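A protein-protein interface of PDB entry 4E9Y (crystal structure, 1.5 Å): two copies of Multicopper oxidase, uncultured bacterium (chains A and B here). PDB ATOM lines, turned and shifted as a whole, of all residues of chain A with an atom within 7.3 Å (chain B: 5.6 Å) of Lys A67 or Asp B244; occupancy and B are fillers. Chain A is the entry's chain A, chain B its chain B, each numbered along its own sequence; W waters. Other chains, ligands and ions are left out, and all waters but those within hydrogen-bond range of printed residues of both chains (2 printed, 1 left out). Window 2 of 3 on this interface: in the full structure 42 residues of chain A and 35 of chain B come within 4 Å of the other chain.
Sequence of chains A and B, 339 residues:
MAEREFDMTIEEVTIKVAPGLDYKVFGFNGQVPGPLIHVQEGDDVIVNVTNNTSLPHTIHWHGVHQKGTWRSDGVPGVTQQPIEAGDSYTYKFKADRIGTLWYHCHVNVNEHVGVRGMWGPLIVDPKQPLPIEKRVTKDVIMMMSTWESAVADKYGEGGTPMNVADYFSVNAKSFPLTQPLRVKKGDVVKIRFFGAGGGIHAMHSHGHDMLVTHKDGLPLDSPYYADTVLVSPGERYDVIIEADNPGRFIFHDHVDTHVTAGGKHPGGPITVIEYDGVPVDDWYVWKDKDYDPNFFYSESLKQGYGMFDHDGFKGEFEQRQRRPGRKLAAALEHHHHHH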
ATOM      1  N   VAL A  64     -11.554 -19.044 -10.753  1.00  0.00           N
ATOM      2  CA  VAL A  64     -10.885 -18.757 -12.024  1.00  0.00           C
ATOM      3  C   VAL A  64     -11.542 -17.538 -12.657  1.00  0.00           C
ATOM      4  O   VAL A  64     -12.764 -17.548 -12.837  1.00  0.00           O
ATOM      5  CB  VAL A  64     -10.969 -19.975 -12.967  1.00  0.00           C
ATOM      6  CG1 VAL A  64     -10.495 -19.637 -14.368  1.00  0.00           C
ATOM      7  CG2 VAL A  64     -10.130 -21.131 -12.400  1.00  0.00           C
ATOM      8  N   HIS A  65     -10.776 -16.505 -12.973  1.00  0.00           N
ATOM      9  CA  HIS A  65     -11.451 -15.297 -13.462  1.00  0.00           C
ATOM     10  C   HIS A  65     -12.065 -15.472 -14.843  1.00  0.00           C
ATOM     11  O   HIS A  65     -13.002 -14.743 -15.173  1.00  0.00           O
ATOM     12  CB  HIS A  65     -10.432 -14.155 -13.501  1.00  0.00           C
ATOM     13  CG  HIS A  65      -9.999 -13.652 -12.157  1.00  0.00           C
ATOM     14  ND1 HIS A  65      -8.869 -12.866 -12.014  1.00  0.00           N
ATOM     15  CD2 HIS A  65     -10.548 -13.799 -10.927  1.00  0.00           C
ATOM     16  CE1 HIS A  65      -8.721 -12.554 -10.738  1.00  0.00           C
ATOM     17  NE2 HIS A  65      -9.716 -13.099 -10.083  1.00  0.00           N
ATOM     18  N   GLN A  66     -11.551 -16.397 -15.648  1.00  0.00           N
ATOM     19  CA  GLN A  66     -12.049 -16.526 -17.021  1.00  0.00           C
ATOM     20  C   GLN A  66     -11.854 -15.219 -17.771  1.00  0.00           C
ATOM     21  O   GLN A  66     -12.749 -14.755 -18.465  1.00  0.00           O
ATOM     22  CB  GLN A  66     -13.511 -16.968 -17.072  1.00  0.00           C
ATOM     23  CG  GLN A  66     -13.792 -18.303 -16.401  1.00  0.00           C
ATOM     24  CD  GLN A  66     -13.184 -19.513 -17.087  1.00  0.00           C
ATOM     25  OE1 GLN A  66     -12.634 -19.444 -18.188  1.00  0.00           O
ATOM     26  NE2 GLN A  66     -13.280 -20.660 -16.397  1.00  0.00           N
ATOM     27  N   LYS A  67     -10.669 -14.640 -17.645  1.00  0.00           N
ATOM     28  CA  LYS A  67     -10.315 -13.375 -18.279  1.00  0.00           C
ATOM     29  C   LYS A  67     -10.358 -13.532 -19.797  1.00  0.00           C
ATOM     30  O   LYS A  67      -9.482 -14.211 -20.343  1.00  0.00           O
ATOM     31  CB  LYS A  67      -8.943 -12.927 -17.793  1.00  0.00           C
ATOM     32  CG  LYS A  67      -8.496 -11.553 -18.230  1.00  0.00           C
ATOM     33  CD  LYS A  67      -9.501 -10.472 -17.853  1.00  0.00           C
ATOM     34  CE  LYS A  67      -8.841  -9.387 -17.005  1.00  0.00           C
ATOM     35  NZ  LYS A  67      -9.019  -9.634 -15.544  1.00  0.00           N
ATOM     36  N   GLY A  68     -11.367 -12.937 -20.412  1.00  0.00           N
ATOM     37  CA  GLY A  68     -11.596 -13.058 -21.842  1.00  0.00           C
ATOM     38  C   GLY A  68     -12.060 -14.446 -22.228  1.00  0.00           C
ATOM     39  O   GLY A  68     -12.045 -14.825 -23.400  1.00  0.00           O
ATOM     40  N   THR A  69     -12.473 -15.283 -21.281  1.00  0.00           N
ATOM     41  CA  THR A  69     -12.894 -16.647 -21.617  1.00  0.00           C
ATOM     42  C   THR A  69     -14.182 -17.003 -20.880  1.00  0.00           C
ATOM     43  O   THR A  69     -14.394 -18.152 -20.497  1.00  0.00           O
ATOM     44  CB  THR A  69     -11.821 -17.716 -21.326  1.00  0.00           C
ATOM     45  OG1 THR A  69     -11.530 -17.789 -19.920  1.00  0.00           O
ATOM     46  CG2 THR A  69     -10.511 -17.349 -22.008  1.00  0.00           C
ATOM     47  N   TRP A  70     -15.056 -16.003 -20.687  1.00  0.00           N
ATOM     48  CA  TRP A  70     -16.287 -16.218 -19.924  1.00  0.00           C
ATOM     49  C   TRP A  70     -17.130 -17.383 -20.400  1.00  0.00           C
ATOM     50  O   TRP A  70     -17.894 -18.022 -19.671  1.00  0.00           O
ATOM     51  CB  TRP A  70     -17.085 -14.900 -19.919  1.00  0.00           C
ATOM     52  CG  TRP A  70     -17.679 -14.462 -21.227  1.00  0.00           C
ATOM     53  CD1 TRP A  70     -17.099 -13.672 -22.169  1.00  0.00           C
ATOM     54  CD2 TRP A  70     -18.980 -14.798 -21.712  1.00  0.00           C
ATOM     55  NE1 TRP A  70     -17.950 -13.486 -23.237  1.00  0.00           N
ATOM     56  CE2 TRP A  70     -19.107 -14.159 -22.986  1.00  0.00           C
ATOM     57  CE3 TRP A  70     -20.066 -15.560 -21.248  1.00  0.00           C
ATOM     58  CZ2 TRP A  70     -20.285 -14.307 -23.711  1.00  0.00           C
ATOM     59  CZ3 TRP A  70     -21.229 -15.688 -21.998  1.00  0.00           C
ATOM     60  CH2 TRP A  70     -21.324 -15.041 -23.255  1.00  0.00           C
ATOM     61  N   PHE A  93      -9.086 -22.207 -20.162  1.00  0.00           N
ATOM     62  CA  PHE A  93      -8.829 -20.978 -19.412  1.00  0.00           C
ATOM     63  C   PHE A  93      -7.368 -20.837 -19.060  1.00  0.00           C
ATOM     64  O   PHE A  93      -6.622 -21.828 -18.969  1.00  0.00           O
ATOM     65  CB  PHE A  93      -9.711 -20.938 -18.162  1.00  0.00           C
ATOM     66  CG  PHE A  93      -9.490 -22.091 -17.185  1.00  0.00           C
ATOM     67  CD1 PHE A  93      -8.531 -22.024 -16.190  1.00  0.00           C
ATOM     68  CD2 PHE A  93     -10.285 -23.221 -17.307  1.00  0.00           C
ATOM     69  CE1 PHE A  93      -8.379 -23.098 -15.330  1.00  0.00           C
ATOM     70  CE2 PHE A  93     -10.120 -24.292 -16.453  1.00  0.00           C
ATOM     71  CZ  PHE A  93      -9.161 -24.230 -15.455  1.00  0.00           C
ATOM     72  N   LYS A  94      -6.927 -19.602 -18.856  1.00  0.00           N
ATOM     73  CA  LYS A  94      -5.567 -19.377 -18.367  1.00  0.00           C
ATOM     74  C   LYS A  94      -5.652 -19.358 -16.845  1.00  0.00           C
ATOM     75  O   LYS A  94      -6.555 -18.749 -16.284  1.00  0.00           O
ATOM     76  CB  LYS A  94      -4.945 -18.096 -18.887  1.00  0.00           C
ATOM     77  CG  LYS A  94      -3.516 -17.778 -18.466  1.00  0.00           C
ATOM     78  CD  LYS A  94      -2.947 -16.635 -19.287  1.00  0.00           C
ATOM     79  CE  LYS A  94      -2.027 -17.156 -20.385  1.00  0.00           C
ATOM     80  NZ  LYS A  94      -0.592 -17.011 -19.974  1.00  0.00           N
ATOM     81  N   ASP A  96      -4.630 -17.605 -14.431  1.00  0.00           N
ATOM     82  CA  ASP A  96      -3.862 -16.458 -13.985  1.00  0.00           C
ATOM     83  C   ASP A  96      -4.211 -16.057 -12.558  1.00  0.00           C
ATOM     84  O   ASP A  96      -3.635 -15.113 -12.019  1.00  0.00           O
ATOM     85  CB  ASP A  96      -4.087 -15.270 -14.923  1.00  0.00           C
ATOM     86  CG  ASP A  96      -5.544 -15.030 -15.259  1.00  0.00           C
ATOM     87  OD1 ASP A  96      -6.441 -15.450 -14.500  1.00  0.00           O
ATOM     88  OD2 ASP A  96      -5.801 -14.402 -16.317  1.00  0.00           O
ATOM     89  N   LYS B 185     -17.292  -2.047 -19.136  1.00  0.00           N
ATOM     90  CA  LYS B 185     -15.878  -2.215 -18.891  1.00  0.00           C
ATOM     91  C   LYS B 185     -15.242  -0.922 -18.378  1.00  0.00           C
ATOM     92  O   LYS B 185     -15.480   0.127 -18.971  1.00  0.00           O
ATOM     93  CB  LYS B 185     -15.157  -2.671 -20.167  1.00  0.00           C
ATOM     94  CG  LYS B 185     -13.659  -2.819 -19.949  1.00  0.00           C
ATOM     95  CD  LYS B 185     -12.990  -3.582 -21.080  1.00  0.00           C
ATOM     96  CE  LYS B 185     -11.476  -3.581 -20.878  1.00  0.00           C
ATOM     97  NZ  LYS B 185     -10.876  -2.359 -21.501  1.00  0.00           N
ATOM     98  N   GLY B 186     -14.475  -1.049 -17.293  1.00  0.00           N
ATOM     99  CA  GLY B 186     -13.799  -0.002 -16.568  1.00  0.00           C
ATOM    100  C   GLY B 186     -14.638   0.610 -15.439  1.00  0.00           C
ATOM    101  O   GLY B 186     -14.145   1.504 -14.731  1.00  0.00           O
ATOM    102  N   ASP B 187     -15.871   0.160 -15.272  1.00  0.00           N
ATOM    103  CA  ASP B 187     -16.684   0.573 -14.130  1.00  0.00           C
ATOM    104  C   ASP B 187     -15.919   0.170 -12.861  1.00  0.00           C
ATOM    105  O   ASP B 187     -15.159  -0.798 -12.845  1.00  0.00           O
ATOM    106  CB  ASP B 187     -18.050  -0.099 -14.097  1.00  0.00           C
ATOM    107  CG  ASP B 187     -19.134   0.764 -14.725  1.00  0.00           C
ATOM    108  OD1 ASP B 187     -18.901   1.992 -14.739  1.00  0.00           O
ATOM    109  OD2 ASP B 187     -20.172   0.229 -15.169  1.00  0.00           O
ATOM    110  N   GLY B 207     -16.062 -14.528 -12.091  1.00  0.00           N
ATOM    111  CA  GLY B 207     -15.329 -13.714 -13.023  1.00  0.00           C
ATOM    112  C   GLY B 207     -14.508 -12.626 -12.382  1.00  0.00           C
ATOM    113  O   GLY B 207     -13.785 -11.888 -13.084  1.00  0.00           O
ATOM    114  N   HIS B 208     -14.627 -12.433 -11.053  1.00  0.00           N
ATOM    115  CA  HIS B 208     -14.041 -11.275 -10.395  1.00  0.00           C
ATOM    116  C   HIS B 208     -13.721 -11.582  -8.910  1.00  0.00           C
ATOM    117  O   HIS B 208     -14.536 -12.302  -8.378  1.00  0.00           O
ATOM    118  CB  HIS B 208     -14.991 -10.079 -10.363  1.00  0.00           C
ATOM    119  CG  HIS B 208     -15.556  -9.618 -11.691  1.00  0.00           C
ATOM    120  ND1 HIS B 208     -16.602 -10.328 -12.276  1.00  0.00           N
ATOM    121  CD2 HIS B 208     -15.255  -8.605 -12.519  1.00  0.00           C
ATOM    122  CE1 HIS B 208     -16.910  -9.729 -13.436  1.00  0.00           C
ATOM    123  NE2 HIS B 208     -16.112  -8.703 -13.590  1.00  0.00           N
ATOM    124  N   GLU B 242     -13.581  -4.324  -9.631  1.00  0.00           N
ATOM    125  CA  GLU B 242     -13.129  -3.646 -10.833  1.00  0.00           C
ATOM    126  C   GLU B 242     -13.770  -4.372 -12.009  1.00  0.00           C
ATOM    127  O   GLU B 242     -13.513  -5.560 -12.178  1.00  0.00           O
ATOM    128  CB  GLU B 242     -11.612  -3.718 -10.928  1.00  0.00           C
ATOM    129  CG  GLU B 242     -10.847  -3.169  -9.741  1.00  0.00           C
ATOM    130  CD  GLU B 242     -10.684  -1.664  -9.749  1.00  0.00           C
ATOM    131  OE1 GLU B 242     -11.001  -0.997 -10.758  1.00  0.00           O
ATOM    132  OE2 GLU B 242     -10.220  -1.136  -8.711  1.00  0.00           O
ATOM    133  N   ALA B 243     -14.592  -3.685 -12.813  1.00  0.00           N
ATOM    134  CA  ALA B 243     -15.302  -4.346 -13.907  1.00  0.00           C
ATOM    135  C   ALA B 243     -14.399  -4.410 -15.126  1.00  0.00           C
ATOM    136  O   ALA B 243     -14.539  -3.669 -16.109  1.00  0.00           O
ATOM    137  CB  ALA B 243     -16.617  -3.616 -14.176  1.00  0.00           C
ATOM    138  N   ASP B 244     -13.409  -5.296 -15.071  1.00  0.00           N
ATOM    139  CA  ASP B 244     -12.418  -5.295 -16.148  1.00  0.00           C
ATOM    140  C   ASP B 244     -12.412  -6.616 -16.908  1.00  0.00           C
ATOM    141  O   ASP B 244     -11.408  -6.944 -17.547  1.00  0.00           O
ATOM    142  CB  ASP B 244     -11.020  -5.040 -15.579  1.00  0.00           C
ATOM    143  CG  ASP B 244     -10.612  -6.109 -14.592  1.00  0.00           C
ATOM    144  OD1 ASP B 244     -11.303  -7.133 -14.367  1.00  0.00           O
ATOM    145  OD2 ASP B 244      -9.527  -5.899 -14.002  1.00  0.00           O
ATOM    146  N   ASN B 245     -13.508  -7.360 -16.856  1.00  0.00           N
ATOM    147  CA  ASN B 245     -13.492  -8.676 -17.508  1.00  0.00           C
ATOM    148  C   ASN B 245     -14.823  -8.924 -18.165  1.00  0.00           C
ATOM    149  O   ASN B 245     -15.712  -9.606 -17.638  1.00  0.00           O
ATOM    150  CB  ASN B 245     -13.203  -9.717 -16.423  1.00  0.00           C
ATOM    151  CG  ASN B 245     -13.183 -11.136 -16.958  1.00  0.00           C
ATOM    152  OD1 ASN B 245     -13.049 -11.319 -18.168  1.00  0.00           O
ATOM    153  ND2 ASN B 245     -13.303 -12.120 -16.066  1.00  0.00           N
ATOM    154  N   PRO B 246     -15.071  -8.331 -19.342  1.00  0.00           N
ATOM    155  CA  PRO B 246     -16.399  -8.456 -19.922  1.00  0.00           C
ATOM    156  C   PRO B 246     -16.888  -9.881 -20.159  1.00  0.00           C
ATOM    157  O   PRO B 246     -16.187 -10.770 -20.656  1.00  0.00           O
ATOM    158  CB  PRO B 246     -16.230  -7.756 -21.281  1.00  0.00           C
ATOM    159  CG  PRO B 246     -15.046  -6.853 -21.140  1.00  0.00           C
ATOM    160  CD  PRO B 246     -14.140  -7.498 -20.105  1.00  0.00           C
ATOM    161  N   TYR B 275     -22.068  -7.332 -18.746  1.00  0.00           N
ATOM    162  CA  TYR B 275     -21.342  -6.211 -19.328  1.00  0.00           C
ATOM    163  C   TYR B 275     -21.972  -5.720 -20.641  1.00  0.00           C
ATOM    164  O   TYR B 275     -22.388  -6.570 -21.434  1.00  0.00           O
ATOM    165  CB  TYR B 275     -19.920  -6.622 -19.644  1.00  0.00           C
ATOM    166  CG  TYR B 275     -18.920  -6.701 -18.522  1.00  0.00           C
ATOM    167  CD1 TYR B 275     -19.041  -7.688 -17.547  1.00  0.00           C
ATOM    168  CD2 TYR B 275     -17.872  -5.812 -18.454  1.00  0.00           C
ATOM    169  CE1 TYR B 275     -18.095  -7.742 -16.507  1.00  0.00           C
ATOM    170  CE2 TYR B 275     -16.919  -5.859 -17.440  1.00  0.00           C
ATOM    171  CZ  TYR B 275     -17.070  -6.850 -16.475  1.00  0.00           C
ATOM    172  OH  TYR B 275     -16.111  -6.857 -15.516  1.00  0.00           O
HETATM  173  O   HOH W   1     -15.485 -17.210 -12.569  1.00  0.00           O
HETATM  174  O   HOH W   2     -11.699  -9.997 -20.125  1.00  0.00           O
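The side-chain amide oxygen (OD1) of Asn B245 lies close to the backbone carbonyl oxygen (O) of Gln A66, 3.5 Å away.
N of Gly A68 is in hydrogen-bond range of OD1 of Asn B245 (3.2 Å).
O of His A65 lies within hydrogen-bond range of ND2 of Asn B245 (2.8 Å).
The side-chain amino group of Lys A67 is in salt-bridge range of the side-chain carboxylate of Asp B244 (3.6 Å).
The side-chain hydroxyl (OG1) of Thr A69 sits at hydrogen-bond distance from the side-chain amide oxygen (OE1) of Gln A66 (2.6 Å).
ND2 of Asn B245 is in hydrogen-bond range of O of Gly B207 (3.0 Å).
The backbone NH (N) of Asn B245 sits at hydrogen-bond distance from the side-chain hydroxyl (OH) of Tyr B275, 3.0 Å away.
The side-chain hydroxyl (OH) of Tyr B275 is in hydrogen-bond range of the backbone NH (N) of Asp B244.
His A65 touches Gly B207.
CA of Lys A67 touches OD1 of Asn B245 (3.4 Å).
Trp A70 touches Pro B246 (CD1 to O, 3.4 Å).
Printed residues of chain B within 4 Å of Gln A66: Asn B245.
Lys A67 touches just these residues of chain B: Asp B244 and Asn B245.
Of the printed residues of chain A, Gly B207 touches His A65.
Of chain A, only Lys A67 comes within 4 Å of Asp B244.
The nearest printed residue of chain B that does not touch Lys A67 is Gly B207 (5.8 Å).
The nearest printed residue of chain A that does not touch Gly B207 is Val A64 (4.5 Å).
Of the 11 printed residues of chain B, 4 touch a printed residue of chain A.
Hydrophobic or aromatic side chains of chain A that line the printed part of chain B: Trp A70.
Among the printed residues, Asp or Glu carboxylates within 4 Å of a Lys or Arg side-chain nitrogen of the other chain: Lys A67 with Asp B244.
No position is printed for both chains.
Of the 7 pairs that touch across the chains among the printed residues, none has its exchanged pair printed and touching as well.
Water W2 bridges the side-chain amide oxygen of Asn B245 and the backbone NH of Gly A68.
Water W1 bridges O of Val A64 and N of Gly B207.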
